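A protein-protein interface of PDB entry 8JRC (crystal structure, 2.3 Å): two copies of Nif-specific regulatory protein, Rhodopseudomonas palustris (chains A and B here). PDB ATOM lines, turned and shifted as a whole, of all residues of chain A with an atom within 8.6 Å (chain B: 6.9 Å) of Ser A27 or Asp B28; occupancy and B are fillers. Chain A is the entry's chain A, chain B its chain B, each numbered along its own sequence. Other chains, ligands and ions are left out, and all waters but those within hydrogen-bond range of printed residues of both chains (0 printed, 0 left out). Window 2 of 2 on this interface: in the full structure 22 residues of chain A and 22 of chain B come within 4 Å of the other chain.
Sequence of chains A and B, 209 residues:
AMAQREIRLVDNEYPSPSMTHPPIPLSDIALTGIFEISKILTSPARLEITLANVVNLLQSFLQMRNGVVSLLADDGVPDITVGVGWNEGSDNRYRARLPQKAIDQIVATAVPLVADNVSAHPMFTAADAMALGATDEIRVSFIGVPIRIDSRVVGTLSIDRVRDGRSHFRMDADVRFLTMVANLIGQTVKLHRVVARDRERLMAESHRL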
ATOM      1  N   PRO A  25      -0.358 -17.230  -5.694  1.00  0.00           N
ATOM      2  CA  PRO A  25      -1.186 -18.158  -6.472  1.00  0.00           C
ATOM      3  C   PRO A  25      -2.409 -17.490  -7.091  1.00  0.00           C
ATOM      4  O   PRO A  25      -3.160 -16.800  -6.398  1.00  0.00           O
ATOM      5  CB  PRO A  25      -1.600 -19.199  -5.433  1.00  0.00           C
ATOM      6  CG  PRO A  25      -0.450 -19.236  -4.489  1.00  0.00           C
ATOM      7  CD  PRO A  25       0.087 -17.827  -4.422  1.00  0.00           C
ATOM      8  N   LEU A  26      -2.593 -17.706  -8.394  1.00  0.00           N
ATOM      9  CA  LEU A  26      -3.754 -17.161  -9.090  1.00  0.00           C
ATOM     10  C   LEU A  26      -5.055 -17.618  -8.439  1.00  0.00           C
ATOM     11  O   LEU A  26      -6.023 -16.853  -8.364  1.00  0.00           O
ATOM     12  CB  LEU A  26      -3.713 -17.567 -10.567  1.00  0.00           C
ATOM     13  CG  LEU A  26      -3.993 -19.037 -10.922  1.00  0.00           C
ATOM     14  CD1 LEU A  26      -4.369 -19.183 -12.391  1.00  0.00           C
ATOM     15  CD2 LEU A  26      -2.825 -19.965 -10.574  1.00  0.00           C
ATOM     16  N   SER A  27      -5.095 -18.862  -7.958  1.00  0.00           N
ATOM     17  CA  SER A  27      -6.305 -19.376  -7.325  1.00  0.00           C
ATOM     18  C   SER A  27      -6.548 -18.721  -5.972  1.00  0.00           C
ATOM     19  O   SER A  27      -7.699 -18.479  -5.593  1.00  0.00           O
ATOM     20  CB  SER A  27      -6.211 -20.891  -7.177  1.00  0.00           C
ATOM     21  OG  SER A  27      -4.994 -21.261  -6.552  1.00  0.00           O
ATOM     22  N   ASP A  28      -5.477 -18.446  -5.224  1.00  0.00           N
ATOM     23  CA  ASP A  28      -5.615 -17.710  -3.972  1.00  0.00           C
ATOM     24  C   ASP A  28      -6.206 -16.330  -4.222  1.00  0.00           C
ATOM     25  O   ASP A  28      -7.139 -15.903  -3.531  1.00  0.00           O
ATOM     26  CB  ASP A  28      -4.256 -17.588  -3.282  1.00  0.00           C
ATOM     27  CG  ASP A  28      -3.835 -18.864  -2.586  1.00  0.00           C
ATOM     28  OD1 ASP A  28      -4.430 -19.923  -2.868  1.00  0.00           O
ATOM     29  OD2 ASP A  28      -2.907 -18.805  -1.753  1.00  0.00           O
ATOM     30  N   ILE A  29      -5.672 -15.620  -5.218  1.00  0.00           N
ATOM     31  CA  ILE A  29      -6.153 -14.282  -5.535  1.00  0.00           C
ATOM     32  C   ILE A  29      -7.587 -14.334  -6.051  1.00  0.00           C
ATOM     33  O   ILE A  29      -8.398 -13.446  -5.762  1.00  0.00           O
ATOM     34  CB  ILE A  29      -5.199 -13.614  -6.542  1.00  0.00           C
ATOM     35  CG1 ILE A  29      -3.799 -13.495  -5.933  1.00  0.00           C
ATOM     36  CG2 ILE A  29      -5.720 -12.252  -6.965  1.00  0.00           C
ATOM     37  CD1 ILE A  29      -2.832 -12.686  -6.764  1.00  0.00           C
ATOM     38  N   ALA A  30      -7.930 -15.380  -6.806  1.00  0.00           N
ATOM     39  CA  ALA A  30      -9.297 -15.507  -7.299  1.00  0.00           C
ATOM     40  C   ALA A  30     -10.261 -15.896  -6.185  1.00  0.00           C
ATOM     41  O   ALA A  30     -11.421 -15.468  -6.194  1.00  0.00           O
ATOM     42  CB  ALA A  30      -9.357 -16.525  -8.437  1.00  0.00           C
ATOM     43  N   LEU A  31      -9.802 -16.702  -5.223  1.00  0.00           N
ATOM     44  CA  LEU A  31     -10.639 -17.029  -4.072  1.00  0.00           C
ATOM     45  C   LEU A  31     -10.955 -15.781  -3.256  1.00  0.00           C
ATOM     46  O   LEU A  31     -12.103 -15.570  -2.850  1.00  0.00           O
ATOM     47  CB  LEU A  31      -9.949 -18.080  -3.202  1.00  0.00           C
ATOM     48  CG  LEU A  31     -10.629 -19.443  -3.058  1.00  0.00           C
ATOM     49  CD1 LEU A  31     -10.063 -20.192  -1.862  1.00  0.00           C
ATOM     50  CD2 LEU A  31     -12.138 -19.293  -2.937  1.00  0.00           C
ATOM     51  N   THR A  32      -9.946 -14.945  -3.005  1.00  0.00           N
ATOM     52  CA  THR A  32     -10.187 -13.684  -2.312  1.00  0.00           C
ATOM     53  C   THR A  32     -11.115 -12.782  -3.116  1.00  0.00           C
ATOM     54  O   THR A  32     -11.944 -12.063  -2.545  1.00  0.00           O
ATOM     55  CB  THR A  32      -8.862 -12.974  -2.035  1.00  0.00           C
ATOM     56  OG1 THR A  32      -7.907 -13.919  -1.533  1.00  0.00           O
ATOM     57  CG2 THR A  32      -9.055 -11.869  -1.010  1.00  0.00           C
ATOM     58  N   GLY A  33     -10.989 -12.806  -4.446  1.00  0.00           N
ATOM     59  CA  GLY A  33     -11.829 -11.957  -5.276  1.00  0.00           C
ATOM     60  C   GLY A  33     -13.302 -12.313  -5.193  1.00  0.00           C
ATOM     61  O   GLY A  33     -14.156 -11.430  -5.089  1.00  0.00           O
ATOM     62  N   ILE A  34     -13.619 -13.610  -5.238  1.00  0.00           N
ATOM     63  CA  ILE A  34     -15.015 -14.027  -5.133  1.00  0.00           C
ATOM     64  C   ILE A  34     -15.510 -13.887  -3.697  1.00  0.00           C
ATOM     65  O   ILE A  34     -16.701 -13.648  -3.463  1.00  0.00           O
ATOM     66  CB  ILE A  34     -15.193 -15.463  -5.664  1.00  0.00           C
ATOM     67  CG1 ILE A  34     -16.667 -15.877  -5.632  1.00  0.00           C
ATOM     68  CG2 ILE A  34     -14.348 -16.450  -4.871  1.00  0.00           C
ATOM     69  CD1 ILE A  34     -17.544 -15.090  -6.579  1.00  0.00           C
ATOM     70  N   PHE A  61      -8.339  -6.194  -8.884  1.00  0.00           N
ATOM     71  CA  PHE A  61      -7.903  -7.448  -8.275  1.00  0.00           C
ATOM     72  C   PHE A  61      -7.331  -8.415  -9.310  1.00  0.00           C
ATOM     73  O   PHE A  61      -6.185  -8.859  -9.188  1.00  0.00           O
ATOM     74  CB  PHE A  61      -9.077  -8.098  -7.534  1.00  0.00           C
ATOM     75  CG  PHE A  61      -8.720  -8.665  -6.194  1.00  0.00           C
ATOM     76  CD1 PHE A  61      -8.256  -9.962  -6.080  1.00  0.00           C
ATOM     77  CD2 PHE A  61      -8.865  -7.906  -5.046  1.00  0.00           C
ATOM     78  CE1 PHE A  61      -7.935 -10.489  -4.846  1.00  0.00           C
ATOM     79  CE2 PHE A  61      -8.547  -8.427  -3.809  1.00  0.00           C
ATOM     80  CZ  PHE A  61      -8.080  -9.721  -3.709  1.00  0.00           C
ATOM     81  N   LEU A  62      -8.119  -8.744 -10.331  1.00  0.00           N
ATOM     82  CA  LEU A  62      -7.781  -9.801 -11.276  1.00  0.00           C
ATOM     83  C   LEU A  62      -7.354  -9.273 -12.640  1.00  0.00           C
ATOM     84  O   LEU A  62      -7.251 -10.059 -13.589  1.00  0.00           O
ATOM     85  CB  LEU A  62      -8.965 -10.754 -11.431  1.00  0.00           C
ATOM     86  CG  LEU A  62      -9.650 -11.123 -10.114  1.00  0.00           C
ATOM     87  CD1 LEU A  62     -11.029 -11.705 -10.368  1.00  0.00           C
ATOM     88  CD2 LEU A  62      -8.787 -12.092  -9.320  1.00  0.00           C
ATOM     89  N   ARG A 170      -5.162 -17.924 -18.280  1.00  0.00           N
ATOM     90  CA  ARG A 170      -5.845 -18.872 -19.148  1.00  0.00           C
ATOM     91  C   ARG A 170      -7.266 -18.399 -19.418  1.00  0.00           C
ATOM     92  O   ARG A 170      -7.996 -18.030 -18.493  1.00  0.00           O
ATOM     93  CB  ARG A 170      -5.859 -20.256 -18.506  1.00  0.00           C
ATOM     94  CG  ARG A 170      -4.578 -21.052 -18.674  1.00  0.00           C
ATOM     95  CD  ARG A 170      -4.539 -22.205 -17.683  1.00  0.00           C
ATOM     96  NE  ARG A 170      -5.836 -22.868 -17.578  1.00  0.00           N
ATOM     97  CZ  ARG A 170      -6.199 -23.648 -16.564  1.00  0.00           C
ATOM     98  NH1 ARG A 170      -5.360 -23.867 -15.560  1.00  0.00           N
ATOM     99  NH2 ARG A 170      -7.400 -24.209 -16.552  1.00  0.00           N
ATOM    100  N   ALA A 173     -10.034 -20.357 -17.565  1.00  0.00           N
ATOM    101  CA  ALA A 173     -10.237 -19.979 -16.169  1.00  0.00           C
ATOM    102  C   ALA A 173     -11.081 -18.717 -16.060  1.00  0.00           C
ATOM    103  O   ALA A 173     -11.965 -18.626 -15.200  1.00  0.00           O
ATOM    104  CB  ALA A 173      -8.892 -19.787 -15.471  1.00  0.00           C
ATOM    105  N   ARG A 176     -14.733 -19.664 -16.685  1.00  0.00           N
ATOM    106  CA  ARG A 176     -15.293 -20.268 -15.480  1.00  0.00           C
ATOM    107  C   ARG A 176     -15.605 -19.210 -14.429  1.00  0.00           C
ATOM    108  O   ARG A 176     -16.730 -19.134 -13.920  1.00  0.00           O
ATOM    109  CB  ARG A 176     -14.325 -21.311 -14.916  1.00  0.00           C
ATOM    110  CG  ARG A 176     -14.343 -22.647 -15.635  1.00  0.00           C
ATOM    111  CD  ARG A 176     -13.536 -23.687 -14.868  1.00  0.00           C
ATOM    112  NE  ARG A 176     -14.379 -24.742 -14.313  1.00  0.00           N
ATOM    113  CZ  ARG A 176     -14.494 -25.004 -13.014  1.00  0.00           C
ATOM    114  NH1 ARG A 176     -13.819 -24.286 -12.126  1.00  0.00           N
ATOM    115  NH2 ARG A 176     -15.285 -25.986 -12.603  1.00  0.00           N
ATOM    116  N   PHE A 177     -14.614 -18.379 -14.095  1.00  0.00           N
ATOM    117  CA  PHE A 177     -14.794 -17.383 -13.042  1.00  0.00           C
ATOM    118  C   PHE A 177     -15.910 -16.402 -13.381  1.00  0.00           C
ATOM    119  O   PHE A 177     -16.745 -16.082 -12.526  1.00  0.00           O
ATOM    120  CB  PHE A 177     -13.481 -16.638 -12.799  1.00  0.00           C
ATOM    121  CG  PHE A 177     -13.468 -15.834 -11.530  1.00  0.00           C
ATOM    122  CD1 PHE A 177     -13.006 -16.389 -10.348  1.00  0.00           C
ATOM    123  CD2 PHE A 177     -13.917 -14.522 -11.519  1.00  0.00           C
ATOM    124  CE1 PHE A 177     -12.991 -15.651  -9.179  1.00  0.00           C
ATOM    125  CE2 PHE A 177     -13.906 -13.781 -10.354  1.00  0.00           C
ATOM    126  CZ  PHE A 177     -13.441 -14.346  -9.182  1.00  0.00           C
ATOM    127  N   PRO B  25      -4.881 -29.166  -4.555  1.00  0.00           N
ATOM    128  CA  PRO B  25      -4.342 -27.900  -4.043  1.00  0.00           C
ATOM    129  C   PRO B  25      -5.452 -26.983  -3.537  1.00  0.00           C
ATOM    130  O   PRO B  25      -6.358 -26.648  -4.301  1.00  0.00           O
ATOM    131  CB  PRO B  25      -3.625 -27.297  -5.259  1.00  0.00           C
ATOM    132  CG  PRO B  25      -3.502 -28.419  -6.255  1.00  0.00           C
ATOM    133  CD  PRO B  25      -4.667 -29.314  -6.003  1.00  0.00           C
ATOM    134  N   LEU B  26      -5.327 -26.557  -2.275  1.00  0.00           N
ATOM    135  CA  LEU B  26      -6.430 -26.024  -1.475  1.00  0.00           C
ATOM    136  C   LEU B  26      -7.373 -25.102  -2.246  1.00  0.00           C
ATOM    137  O   LEU B  26      -8.578 -25.362  -2.339  1.00  0.00           O
ATOM    138  CB  LEU B  26      -5.839 -25.296  -0.259  1.00  0.00           C
ATOM    139  CG  LEU B  26      -6.728 -24.692   0.838  1.00  0.00           C
ATOM    140  CD1 LEU B  26      -7.094 -23.244   0.518  1.00  0.00           C
ATOM    141  CD2 LEU B  26      -7.978 -25.529   1.095  1.00  0.00           C
ATOM    142  N   SER B  27      -6.836 -24.019  -2.809  1.00  0.00           N
ATOM    143  CA  SER B  27      -7.687 -22.985  -3.397  1.00  0.00           C
ATOM    144  C   SER B  27      -8.364 -23.445  -4.683  1.00  0.00           C
ATOM    145  O   SER B  27      -9.472 -22.989  -4.989  1.00  0.00           O
ATOM    146  CB  SER B  27      -6.873 -21.721  -3.651  1.00  0.00           C
ATOM    147  OG  SER B  27      -6.247 -21.282  -2.459  1.00  0.00           O
ATOM    148  N   ASP B  28      -7.719 -24.326  -5.453  1.00  0.00           N
ATOM    149  CA  ASP B  28      -8.361 -24.876  -6.644  1.00  0.00           C
ATOM    150  C   ASP B  28      -9.638 -25.621  -6.280  1.00  0.00           C
ATOM    151  O   ASP B  28     -10.685 -25.433  -6.912  1.00  0.00           O
ATOM    152  CB  ASP B  28      -7.400 -25.807  -7.384  1.00  0.00           C
ATOM    153  CG  ASP B  28      -6.178 -25.090  -7.915  1.00  0.00           C
ATOM    154  OD1 ASP B  28      -6.042 -23.879  -7.668  1.00  0.00           O
ATOM    155  OD2 ASP B  28      -5.355 -25.739  -8.595  1.00  0.00           O
ATOM    156  N   ILE B  29      -9.565 -26.478  -5.259  1.00  0.00           N
ATOM    157  CA  ILE B  29     -10.733 -27.243  -4.828  1.00  0.00           C
ATOM    158  C   ILE B  29     -11.836 -26.302  -4.359  1.00  0.00           C
ATOM    159  O   ILE B  29     -13.002 -26.440  -4.748  1.00  0.00           O
ATOM    160  CB  ILE B  29     -10.339 -28.243  -3.727  1.00  0.00           C
ATOM    161  CG1 ILE B  29      -9.156 -29.102  -4.182  1.00  0.00           C
ATOM    162  CG2 ILE B  29     -11.530 -29.106  -3.339  1.00  0.00           C
ATOM    163  CD1 ILE B  29      -9.545 -30.266  -5.070  1.00  0.00           C
ATOM    164  N   ALA B  30     -11.480 -25.330  -3.515  1.00  0.00           N
ATOM    165  CA  ALA B  30     -12.469 -24.374  -3.026  1.00  0.00           C
ATOM    166  C   ALA B  30     -13.074 -23.567  -4.169  1.00  0.00           C
ATOM    167  O   ALA B  30     -14.279 -23.292  -4.172  1.00  0.00           O
ATOM    168  CB  ALA B  30     -11.836 -23.449  -1.988  1.00  0.00           C
ATOM    169  N   LEU B  31     -12.250 -23.176  -5.146  1.00  0.00           N
ATOM    170  CA  LEU B  31     -12.755 -22.432  -6.297  1.00  0.00           C
ATOM    171  C   LEU B  31     -13.797 -23.242  -7.058  1.00  0.00           C
ATOM    172  O   LEU B  31     -14.855 -22.723  -7.430  1.00  0.00           O
ATOM    173  CB  LEU B  31     -11.599 -22.042  -7.218  1.00  0.00           C
ATOM    174  CG  LEU B  31     -11.045 -20.621  -7.095  1.00  0.00           C
ATOM    175  CD1 LEU B  31     -10.173 -20.285  -8.296  1.00  0.00           C
ATOM    176  CD2 LEU B  31     -12.171 -19.608  -6.943  1.00  0.00           C
ATOM    177  N   THR B  32     -13.508 -24.521  -7.306  1.00  0.00           N
ATOM    178  CA  THR B  32     -14.493 -25.389  -7.941  1.00  0.00           C
ATOM    179  C   THR B  32     -15.749 -25.512  -7.088  1.00  0.00           C
ATOM    180  O   THR B  32     -16.869 -25.502  -7.612  1.00  0.00           O
ATOM    181  CB  THR B  32     -13.887 -26.768  -8.203  1.00  0.00           C
ATOM    182  OG1 THR B  32     -12.675 -26.625  -8.955  1.00  0.00           O
ATOM    183  CG2 THR B  32     -14.860 -27.641  -8.979  1.00  0.00           C
ATOM    184  N   GLY B  33     -15.579 -25.628  -5.769  1.00  0.00           N
ATOM    185  CA  GLY B  33     -16.730 -25.743  -4.888  1.00  0.00           C
ATOM    186  C   GLY B  33     -17.643 -24.534  -4.956  1.00  0.00           C
ATOM    187  O   GLY B  33     -18.859 -24.668  -5.119  1.00  0.00           O
ATOM    188  N   PHE B  61     -17.825 -32.903  -1.261  1.00  0.00           N
ATOM    189  CA  PHE B  61     -16.752 -32.354  -2.080  1.00  0.00           C
ATOM    190  C   PHE B  61     -15.668 -31.655  -1.271  1.00  0.00           C
ATOM    191  O   PHE B  61     -14.480 -31.856  -1.539  1.00  0.00           O
ATOM    192  CB  PHE B  61     -17.326 -31.377  -3.111  1.00  0.00           C
ATOM    193  CG  PHE B  61     -16.340 -30.958  -4.165  1.00  0.00           C
ATOM    194  CD1 PHE B  61     -15.850 -31.877  -5.080  1.00  0.00           C
ATOM    195  CD2 PHE B  61     -15.906 -29.646  -4.241  1.00  0.00           C
ATOM    196  CE1 PHE B  61     -14.944 -31.495  -6.049  1.00  0.00           C
ATOM    197  CE2 PHE B  61     -14.999 -29.257  -5.210  1.00  0.00           C
ATOM    198  CZ  PHE B  61     -14.518 -30.182  -6.115  1.00  0.00           C
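The side-chain carboxylate of Asp B28 lies within hydrogen-bond range of the side-chain hydroxyl of Ser A27, 3.0 Å away.
The side-chain hydroxyl (OG) of Ser B27 sits close to the side-chain carboxylate (OD1) of Asp A28 (2.3 Å).
Among the printed residues, merely in contact across the chains: Ser A27 with Ser B27 (3.5 Å), Ala A30 with Leu B31 (3.9 Å), Leu A31 with Ser B27 (3.96 Å) and Leu A31 with Ala B30 (3.7 Å).
Ser A27 touches its own counterpart, Ser B27.
Ser A27 touches Asp B28, and with the chains exchanged Asp A28 touches Ser B27.
Ala A30 touches Leu B31, and with the chains exchanged Leu A31 touches Ala B30.
Leu A31 touches Ser B27, but with the chains exchanged Ser A27 does not touch Leu B31 (4.1 Å).
Asp B28 touches one residue of chain A.
Of the printed residues of chain A, Ala B30 touches Leu A31 (3.7 Å).
Of the printed residues of chain B, Leu A31 touches Ser B27 and Ala B30.
Printed residues of chain A within 4 Å of Leu B31: Ala A30 (3.9 Å).
Printed residues of chain B within 4 Å of Ala A30: Leu B31.
Printed residues of chain B within 4 Å of Asp A28: Ser B27 (2.3 Å).
Thr B32 touches none of the printed residues of chain A.
The nearest residue of chain B that does not touch Ser A27 is Leu B31 (4.1 Å).
The nearest residue of chain A that does not touch Asp B28 is Leu A26 (5.8 Å).
The nearest printed residue of chain B that does not touch Leu A31 is Leu B31 (4.02 Å).
O of Asp A28 sits at hydrogen-bond distance from OG1 of Thr A32 (2.9 Å).
The backbone carbonyl oxygen (O) of Asp B28 sits at hydrogen-bond distance from the side-chain hydroxyl (OG1) of Thr B32, 3.1 Å away.
Of the 10 printed residues of chain B, 4 touch a printed residue of chain A.
Hydrophobic or aromatic side chains of chain B that line the printed part of chain A: Ala B30 and Leu B31.
Of the 16 printed residues of chain A, 4 touch a printed residue of chain B.
Printed residues of chain A that touch a printed residue of chain B: Ser A27, Asp A28, Ala A30 and Leu A31.
Hydrophobic or aromatic side chains of chain A within 4 Å of the printed part of chain B: Ala A30 and Leu A31.
Among the printed residues, 6 pairs touch across the chains.
Among the printed residues, no Asp or Glu carboxylate lies within 4 Å of a Lys or Arg side-chain nitrogen of the other chain.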
